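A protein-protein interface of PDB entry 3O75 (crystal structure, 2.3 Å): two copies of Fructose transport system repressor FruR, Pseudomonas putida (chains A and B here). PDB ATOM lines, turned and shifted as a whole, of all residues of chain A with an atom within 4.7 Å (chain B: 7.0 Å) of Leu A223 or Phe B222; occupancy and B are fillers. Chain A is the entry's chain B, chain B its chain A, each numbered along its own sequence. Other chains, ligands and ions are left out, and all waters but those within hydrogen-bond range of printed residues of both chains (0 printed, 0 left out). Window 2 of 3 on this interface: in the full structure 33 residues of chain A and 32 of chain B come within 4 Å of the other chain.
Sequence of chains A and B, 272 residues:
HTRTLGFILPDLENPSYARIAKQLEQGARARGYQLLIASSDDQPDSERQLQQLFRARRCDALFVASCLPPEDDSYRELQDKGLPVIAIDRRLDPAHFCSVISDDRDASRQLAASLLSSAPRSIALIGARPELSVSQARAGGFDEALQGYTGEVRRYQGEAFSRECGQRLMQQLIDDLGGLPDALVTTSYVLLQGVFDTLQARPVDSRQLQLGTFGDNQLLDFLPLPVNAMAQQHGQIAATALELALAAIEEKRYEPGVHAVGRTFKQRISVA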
ATOM      1  N   PHE A 196      22.375  20.906  16.420  1.00  0.00           N
ATOM      2  CA  PHE A 196      23.387  21.037  17.466  1.00  0.00           C
ATOM      3  C   PHE A 196      23.308  19.871  18.445  1.00  0.00           C
ATOM      4  O   PHE A 196      24.334  19.358  18.886  1.00  0.00           O
ATOM      5  CB  PHE A 196      23.255  22.365  18.222  1.00  0.00           C
ATOM      6  CG  PHE A 196      23.738  23.560  17.446  1.00  0.00           C
ATOM      7  CD1 PHE A 196      23.145  24.802  17.624  1.00  0.00           C
ATOM      8  CD2 PHE A 196      24.772  23.440  16.534  1.00  0.00           C
ATOM      9  CE1 PHE A 196      23.582  25.910  16.910  1.00  0.00           C
ATOM     10  CE2 PHE A 196      25.216  24.541  15.812  1.00  0.00           C
ATOM     11  CZ  PHE A 196      24.620  25.780  15.999  1.00  0.00           C
ATOM     12  N   GLN A 200      26.287  17.315  19.201  1.00  0.00           N
ATOM     13  CA  GLN A 200      26.658  17.216  20.604  1.00  0.00           C
ATOM     14  C   GLN A 200      26.848  15.765  21.024  1.00  0.00           C
ATOM     15  O   GLN A 200      27.789  15.434  21.745  1.00  0.00           O
ATOM     16  CB  GLN A 200      25.572  17.860  21.465  1.00  0.00           C
ATOM     17  CG  GLN A 200      26.042  19.043  22.283  1.00  0.00           C
ATOM     18  CD  GLN A 200      26.534  18.640  23.655  1.00  0.00           C
ATOM     19  OE1 GLN A 200      26.252  17.539  24.126  1.00  0.00           O
ATOM     20  NE2 GLN A 200      27.269  19.533  24.307  1.00  0.00           N
ATOM     21  N   LEU A 219      23.590  32.777  20.945  1.00  0.00           N
ATOM     22  CA  LEU A 219      24.448  31.613  21.112  1.00  0.00           C
ATOM     23  C   LEU A 219      25.577  31.617  20.089  1.00  0.00           C
ATOM     24  O   LEU A 219      26.735  31.385  20.427  1.00  0.00           O
ATOM     25  CB  LEU A 219      23.617  30.333  20.978  1.00  0.00           C
ATOM     26  CG  LEU A 219      24.261  28.973  21.268  1.00  0.00           C
ATOM     27  CD1 LEU A 219      23.203  27.878  21.300  1.00  0.00           C
ATOM     28  CD2 LEU A 219      25.338  28.635  20.253  1.00  0.00           C
ATOM     29  N   LEU A 220      25.231  31.892  18.837  1.00  0.00           N
ATOM     30  CA  LEU A 220      26.189  31.797  17.742  1.00  0.00           C
ATOM     31  C   LEU A 220      27.390  32.731  17.898  1.00  0.00           C
ATOM     32  O   LEU A 220      28.413  32.553  17.233  1.00  0.00           O
ATOM     33  CB  LEU A 220      25.487  32.027  16.401  1.00  0.00           C
ATOM     34  CG  LEU A 220      24.866  30.782  15.759  1.00  0.00           C
ATOM     35  CD1 LEU A 220      24.382  29.799  16.818  1.00  0.00           C
ATOM     36  CD2 LEU A 220      23.730  31.166  14.819  1.00  0.00           C
ATOM     37  N   ASP A 221      27.267  33.721  18.776  1.00  0.00           N
ATOM     38  CA  ASP A 221      28.371  34.637  19.048  1.00  0.00           C
ATOM     39  C   ASP A 221      29.426  33.998  19.946  1.00  0.00           C
ATOM     40  O   ASP A 221      30.524  34.530  20.102  1.00  0.00           O
ATOM     41  CB  ASP A 221      27.856  35.928  19.689  1.00  0.00           C
ATOM     42  CG  ASP A 221      27.126  36.821  18.701  1.00  0.00           C
ATOM     43  OD1 ASP A 221      26.263  37.611  19.139  1.00  0.00           O
ATOM     44  OD2 ASP A 221      27.413  36.732  17.488  1.00  0.00           O
ATOM     45  N   PHE A 222      29.087  32.853  20.529  1.00  0.00           N
ATOM     46  CA  PHE A 222      29.946  32.214  21.521  1.00  0.00           C
ATOM     47  C   PHE A 222      30.449  30.850  21.068  1.00  0.00           C
ATOM     48  O   PHE A 222      31.473  30.366  21.549  1.00  0.00           O
ATOM     49  CB  PHE A 222      29.202  32.068  22.850  1.00  0.00           C
ATOM     50  CG  PHE A 222      28.973  33.368  23.566  1.00  0.00           C
ATOM     51  CD1 PHE A 222      27.799  34.077  23.387  1.00  0.00           C
ATOM     52  CD2 PHE A 222      29.933  33.876  24.426  1.00  0.00           C
ATOM     53  CE1 PHE A 222      27.588  35.272  24.048  1.00  0.00           C
ATOM     54  CE2 PHE A 222      29.727  35.072  25.091  1.00  0.00           C
ATOM     55  CZ  PHE A 222      28.551  35.771  24.901  1.00  0.00           C
ATOM     56  N   LEU A 223      29.722  30.228  20.149  1.00  0.00           N
ATOM     57  CA  LEU A 223      30.059  28.889  19.689  1.00  0.00           C
ATOM     58  C   LEU A 223      31.400  28.854  18.958  1.00  0.00           C
ATOM     59  O   LEU A 223      31.649  29.676  18.072  1.00  0.00           O
ATOM     60  CB  LEU A 223      28.956  28.357  18.776  1.00  0.00           C
ATOM     61  CG  LEU A 223      28.615  26.881  18.948  1.00  0.00           C
ATOM     62  CD1 LEU A 223      28.145  26.645  20.360  1.00  0.00           C
ATOM     63  CD2 LEU A 223      27.553  26.457  17.956  1.00  0.00           C
ATOM     64  N   PRO A 224      32.271  27.899  19.327  1.00  0.00           N
ATOM     65  CA  PRO A 224      33.544  27.732  18.618  1.00  0.00           C
ATOM     66  C   PRO A 224      33.309  27.649  17.116  1.00  0.00           C
ATOM     67  O   PRO A 224      33.959  28.353  16.341  1.00  0.00           O
ATOM     68  CB  PRO A 224      34.050  26.385  19.134  1.00  0.00           C
ATOM     69  CG  PRO A 224      33.478  26.277  20.502  1.00  0.00           C
ATOM     70  CD  PRO A 224      32.137  26.963  20.457  1.00  0.00           C
ATOM     71  N   LEU A 225      32.373  26.794  16.720  1.00  0.00           N
ATOM     72  CA  LEU A 225      32.021  26.626  15.317  1.00  0.00           C
ATOM     73  C   LEU A 225      31.332  27.881  14.784  1.00  0.00           C
ATOM     74  O   LEU A 225      30.314  28.307  15.326  1.00  0.00           O
ATOM     75  CB  LEU A 225      31.116  25.403  15.152  1.00  0.00           C
ATOM     76  CG  LEU A 225      30.644  24.997  13.754  1.00  0.00           C
ATOM     77  CD1 LEU A 225      31.821  24.794  12.810  1.00  0.00           C
ATOM     78  CD2 LEU A 225      29.797  23.734  13.842  1.00  0.00           C
ATOM     79  N   PRO A 226      31.897  28.483  13.726  1.00  0.00           N
ATOM     80  CA  PRO A 226      31.325  29.673  13.086  1.00  0.00           C
ATOM     81  C   PRO A 226      30.107  29.326  12.236  1.00  0.00           C
ATOM     82  O   PRO A 226      30.101  28.277  11.593  1.00  0.00           O
ATOM     83  CB  PRO A 226      32.464  30.166  12.191  1.00  0.00           C
ATOM     84  CG  PRO A 226      33.242  28.940  11.876  1.00  0.00           C
ATOM     85  CD  PRO A 226      33.170  28.078  13.104  1.00  0.00           C
ATOM     86  N   ASN B 217      19.161  27.653  29.201  1.00  0.00           N
ATOM     87  CA  ASN B 217      19.169  27.821  27.749  1.00  0.00           C
ATOM     88  C   ASN B 217      20.129  26.844  27.083  1.00  0.00           C
ATOM     89  O   ASN B 217      21.143  26.467  27.675  1.00  0.00           O
ATOM     90  CB  ASN B 217      19.538  29.263  27.379  1.00  0.00           C
ATOM     91  CG  ASN B 217      19.372  29.551  25.892  1.00  0.00           C
ATOM     92  OD1 ASN B 217      20.278  29.311  25.094  1.00  0.00           O
ATOM     93  ND2 ASN B 217      18.208  30.071  25.519  1.00  0.00           N
ATOM     94  N   GLN B 218      19.808  26.440  25.856  1.00  0.00           N
ATOM     95  CA  GLN B 218      20.634  25.489  25.123  1.00  0.00           C
ATOM     96  C   GLN B 218      22.073  25.978  25.083  1.00  0.00           C
ATOM     97  O   GLN B 218      23.015  25.196  25.204  1.00  0.00           O
ATOM     98  CB  GLN B 218      20.111  25.304  23.697  1.00  0.00           C
ATOM     99  CG  GLN B 218      20.755  24.140  22.949  1.00  0.00           C
ATOM    100  CD  GLN B 218      20.300  24.040  21.507  1.00  0.00           C
ATOM    101  OE1 GLN B 218      19.887  25.032  20.903  1.00  0.00           O
ATOM    102  NE2 GLN B 218      20.383  22.840  20.941  1.00  0.00           N
ATOM    103  N   LEU B 219      22.230  27.285  24.924  1.00  0.00           N
ATOM    104  CA  LEU B 219      23.545  27.908  24.841  1.00  0.00           C
ATOM    105  C   LEU B 219      24.451  27.545  26.023  1.00  0.00           C
ATOM    106  O   LEU B 219      25.668  27.449  25.870  1.00  0.00           O
ATOM    107  CB  LEU B 219      23.390  29.430  24.703  1.00  0.00           C
ATOM    108  CG  LEU B 219      24.446  30.403  25.229  1.00  0.00           C
ATOM    109  CD1 LEU B 219      24.290  31.763  24.568  1.00  0.00           C
ATOM    110  CD2 LEU B 219      24.324  30.553  26.730  1.00  0.00           C
ATOM    111  N   LEU B 220      23.859  27.337  27.194  1.00  0.00           N
ATOM    112  CA  LEU B 220      24.633  27.038  28.397  1.00  0.00           C
ATOM    113  C   LEU B 220      25.274  25.649  28.367  1.00  0.00           C
ATOM    114  O   LEU B 220      26.113  25.326  29.208  1.00  0.00           O
ATOM    115  CB  LEU B 220      23.762  27.193  29.644  1.00  0.00           C
ATOM    116  CG  LEU B 220      23.256  28.609  29.918  1.00  0.00           C
ATOM    117  CD1 LEU B 220      22.513  28.661  31.242  1.00  0.00           C
ATOM    118  CD2 LEU B 220      24.415  29.597  29.913  1.00  0.00           C
ATOM    119  N   ASP B 221      24.868  24.831  27.403  1.00  0.00           N
ATOM    120  CA  ASP B 221      25.427  23.492  27.244  1.00  0.00           C
ATOM    121  C   ASP B 221      26.669  23.501  26.359  1.00  0.00           C
ATOM    122  O   ASP B 221      27.458  22.555  26.372  1.00  0.00           O
ATOM    123  CB  ASP B 221      24.381  22.546  26.659  1.00  0.00           C
ATOM    124  CG  ASP B 221      23.209  22.330  27.588  1.00  0.00           C
ATOM    125  OD1 ASP B 221      22.062  22.521  27.136  1.00  0.00           O
ATOM    126  OD2 ASP B 221      23.435  21.973  28.766  1.00  0.00           O
ATOM    127  N   PHE B 222      26.831  24.570  25.584  1.00  0.00           N
ATOM    128  CA  PHE B 222      27.950  24.676  24.656  1.00  0.00           C
ATOM    129  C   PHE B 222      28.989  25.690  25.116  1.00  0.00           C
ATOM    130  O   PHE B 222      30.097  25.730  24.584  1.00  0.00           O
ATOM    131  CB  PHE B 222      27.459  25.056  23.259  1.00  0.00           C
ATOM    132  CG  PHE B 222      26.504  24.066  22.660  1.00  0.00           C
ATOM    133  CD1 PHE B 222      25.135  24.258  22.754  1.00  0.00           C
ATOM    134  CD2 PHE B 222      26.974  22.948  21.994  1.00  0.00           C
ATOM    135  CE1 PHE B 222      24.254  23.348  22.201  1.00  0.00           C
ATOM    136  CE2 PHE B 222      26.098  22.037  21.437  1.00  0.00           C
ATOM    137  CZ  PHE B 222      24.735  22.236  21.543  1.00  0.00           C
ATOM    138  N   LEU B 223      28.623  26.517  26.090  1.00  0.00           N
ATOM    139  CA  LEU B 223      29.538  27.521  26.612  1.00  0.00           C
ATOM    140  C   LEU B 223      30.755  26.841  27.209  1.00  0.00           C
ATOM    141  O   LEU B 223      30.628  25.823  27.885  1.00  0.00           O
ATOM    142  CB  LEU B 223      28.856  28.362  27.690  1.00  0.00           C
ATOM    143  CG  LEU B 223      28.885  29.877  27.491  1.00  0.00           C
ATOM    144  CD1 LEU B 223      27.583  30.347  26.879  1.00  0.00           C
ATOM    145  CD2 LEU B 223      29.135  30.592  28.806  1.00  0.00           C
ATOM    146  N   PRO B 224      31.944  27.402  26.961  1.00  0.00           N
ATOM    147  CA  PRO B 224      33.149  26.900  27.627  1.00  0.00           C
ATOM    148  C   PRO B 224      33.023  27.160  29.121  1.00  0.00           C
ATOM    149  O   PRO B 224      33.396  26.329  29.948  1.00  0.00           O
ATOM    150  CB  PRO B 224      34.261  27.763  27.027  1.00  0.00           C
ATOM    151  CG  PRO B 224      33.574  29.021  26.594  1.00  0.00           C
ATOM    152  CD  PRO B 224      32.208  28.602  26.148  1.00  0.00           C
ATOM    153  N   LEU B 225      32.482  28.330  29.445  1.00  0.00           N
ATOM    154  CA  LEU B 225      32.209  28.732  30.817  1.00  0.00           C
ATOM    155  C   LEU B 225      30.934  28.064  31.332  1.00  0.00           C
ATOM    156  O   LEU B 225      29.837  28.380  30.874  1.00  0.00           O
ATOM    157  CB  LEU B 225      32.058  30.253  30.874  1.00  0.00           C
ATOM    158  CG  LEU B 225      31.723  30.914  32.208  1.00  0.00           C
ATOM    159  CD1 LEU B 225      32.904  30.815  33.157  1.00  0.00           C
ATOM    160  CD2 LEU B 225      31.334  32.367  31.982  1.00  0.00           C
ATOM    161  N   ARG B 268      26.190  22.623  36.434  1.00  0.00           N
ATOM    162  CA  ARG B 268      27.278  22.415  35.483  1.00  0.00           C
ATOM    163  C   ARG B 268      28.646  22.677  36.111  1.00  0.00           C
ATOM    164  O   ARG B 268      29.663  22.156  35.647  1.00  0.00           O
ATOM    165  CB  ARG B 268      27.086  23.308  34.259  1.00  0.00           C
ATOM    166  CG  ARG B 268      25.775  23.082  33.536  1.00  0.00           C
ATOM    167  CD  ARG B 268      25.645  23.999  32.339  1.00  0.00           C
ATOM    168  NE  ARG B 268      24.487  23.660  31.519  1.00  0.00           N
ATOM    169  CZ  ARG B 268      23.281  24.204  31.658  1.00  0.00           C
ATOM    170  NH1 ARG B 268      23.062  25.125  32.588  1.00  0.00           N
ATOM    171  NH2 ARG B 268      22.294  23.824  30.860  1.00  0.00           N
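Among the printed residues, pairs that only touch across the chains: Gln A200 with Phe B222 (3.1 Å), Leu A223 with Phe B222 (3.4 Å), Leu A219 with Leu B219 (3.5 Å), Phe A196 with Phe B222 (3.6 Å), Gln A200 with Asp B221 (3.7 Å) and Phe A196 with Gln B218 (3.98 Å).
Hydrophobic or aromatic side chains of chain B within 4 Å of the printed part of chain A: Leu B219 and Phe B222. Printed residues of chain A that touch a printed residue of chain B: Phe A196, Gln A200, Leu A219 and Leu A223. Hydrophobic or aromatic side chains of chain A that line the printed part of chain B: Phe A196, Leu A219 and Leu A223. Among the printed residues, no Asp or Glu carboxylate lies within 4 Å of a Lys or Arg side-chain nitrogen of the other chain.
Phe B222 touches three residues of chain A. Printed residues of chain B within 4 Å of Phe A196: Gln B218 and Phe B222. Of the printed residues of chain A, Leu B219 touches Leu A219. Printed residues of chain B within 4 Å of Leu A219: Leu B219 (3.5 Å). Of the printed residues of chain A, Asp B221 touches Gln A200 (3.7 Å). The nearest residue of chain B that does not touch Leu A223 is Leu B223 (5.8 Å). The nearest residue of chain A that does not touch Phe B222 is Leu A219 (4.4 Å).
Leu A219 touches its own counterpart, Leu B219. Leu A223 touches Phe B222, but with the chains exchanged Phe A222 does not touch Leu B223 (4.7 Å). Of the 6 pairs that touch across the chains among the printed residues, 1 has its exchanged pair printed and touching as well.
OD1 of Asn B217 lies within hydrogen-bond range of N of Leu B219 (2.8 Å). OD2 of Asp B221 lies within salt-bridge range of NH2 of Arg B268, 3.0 Å away.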
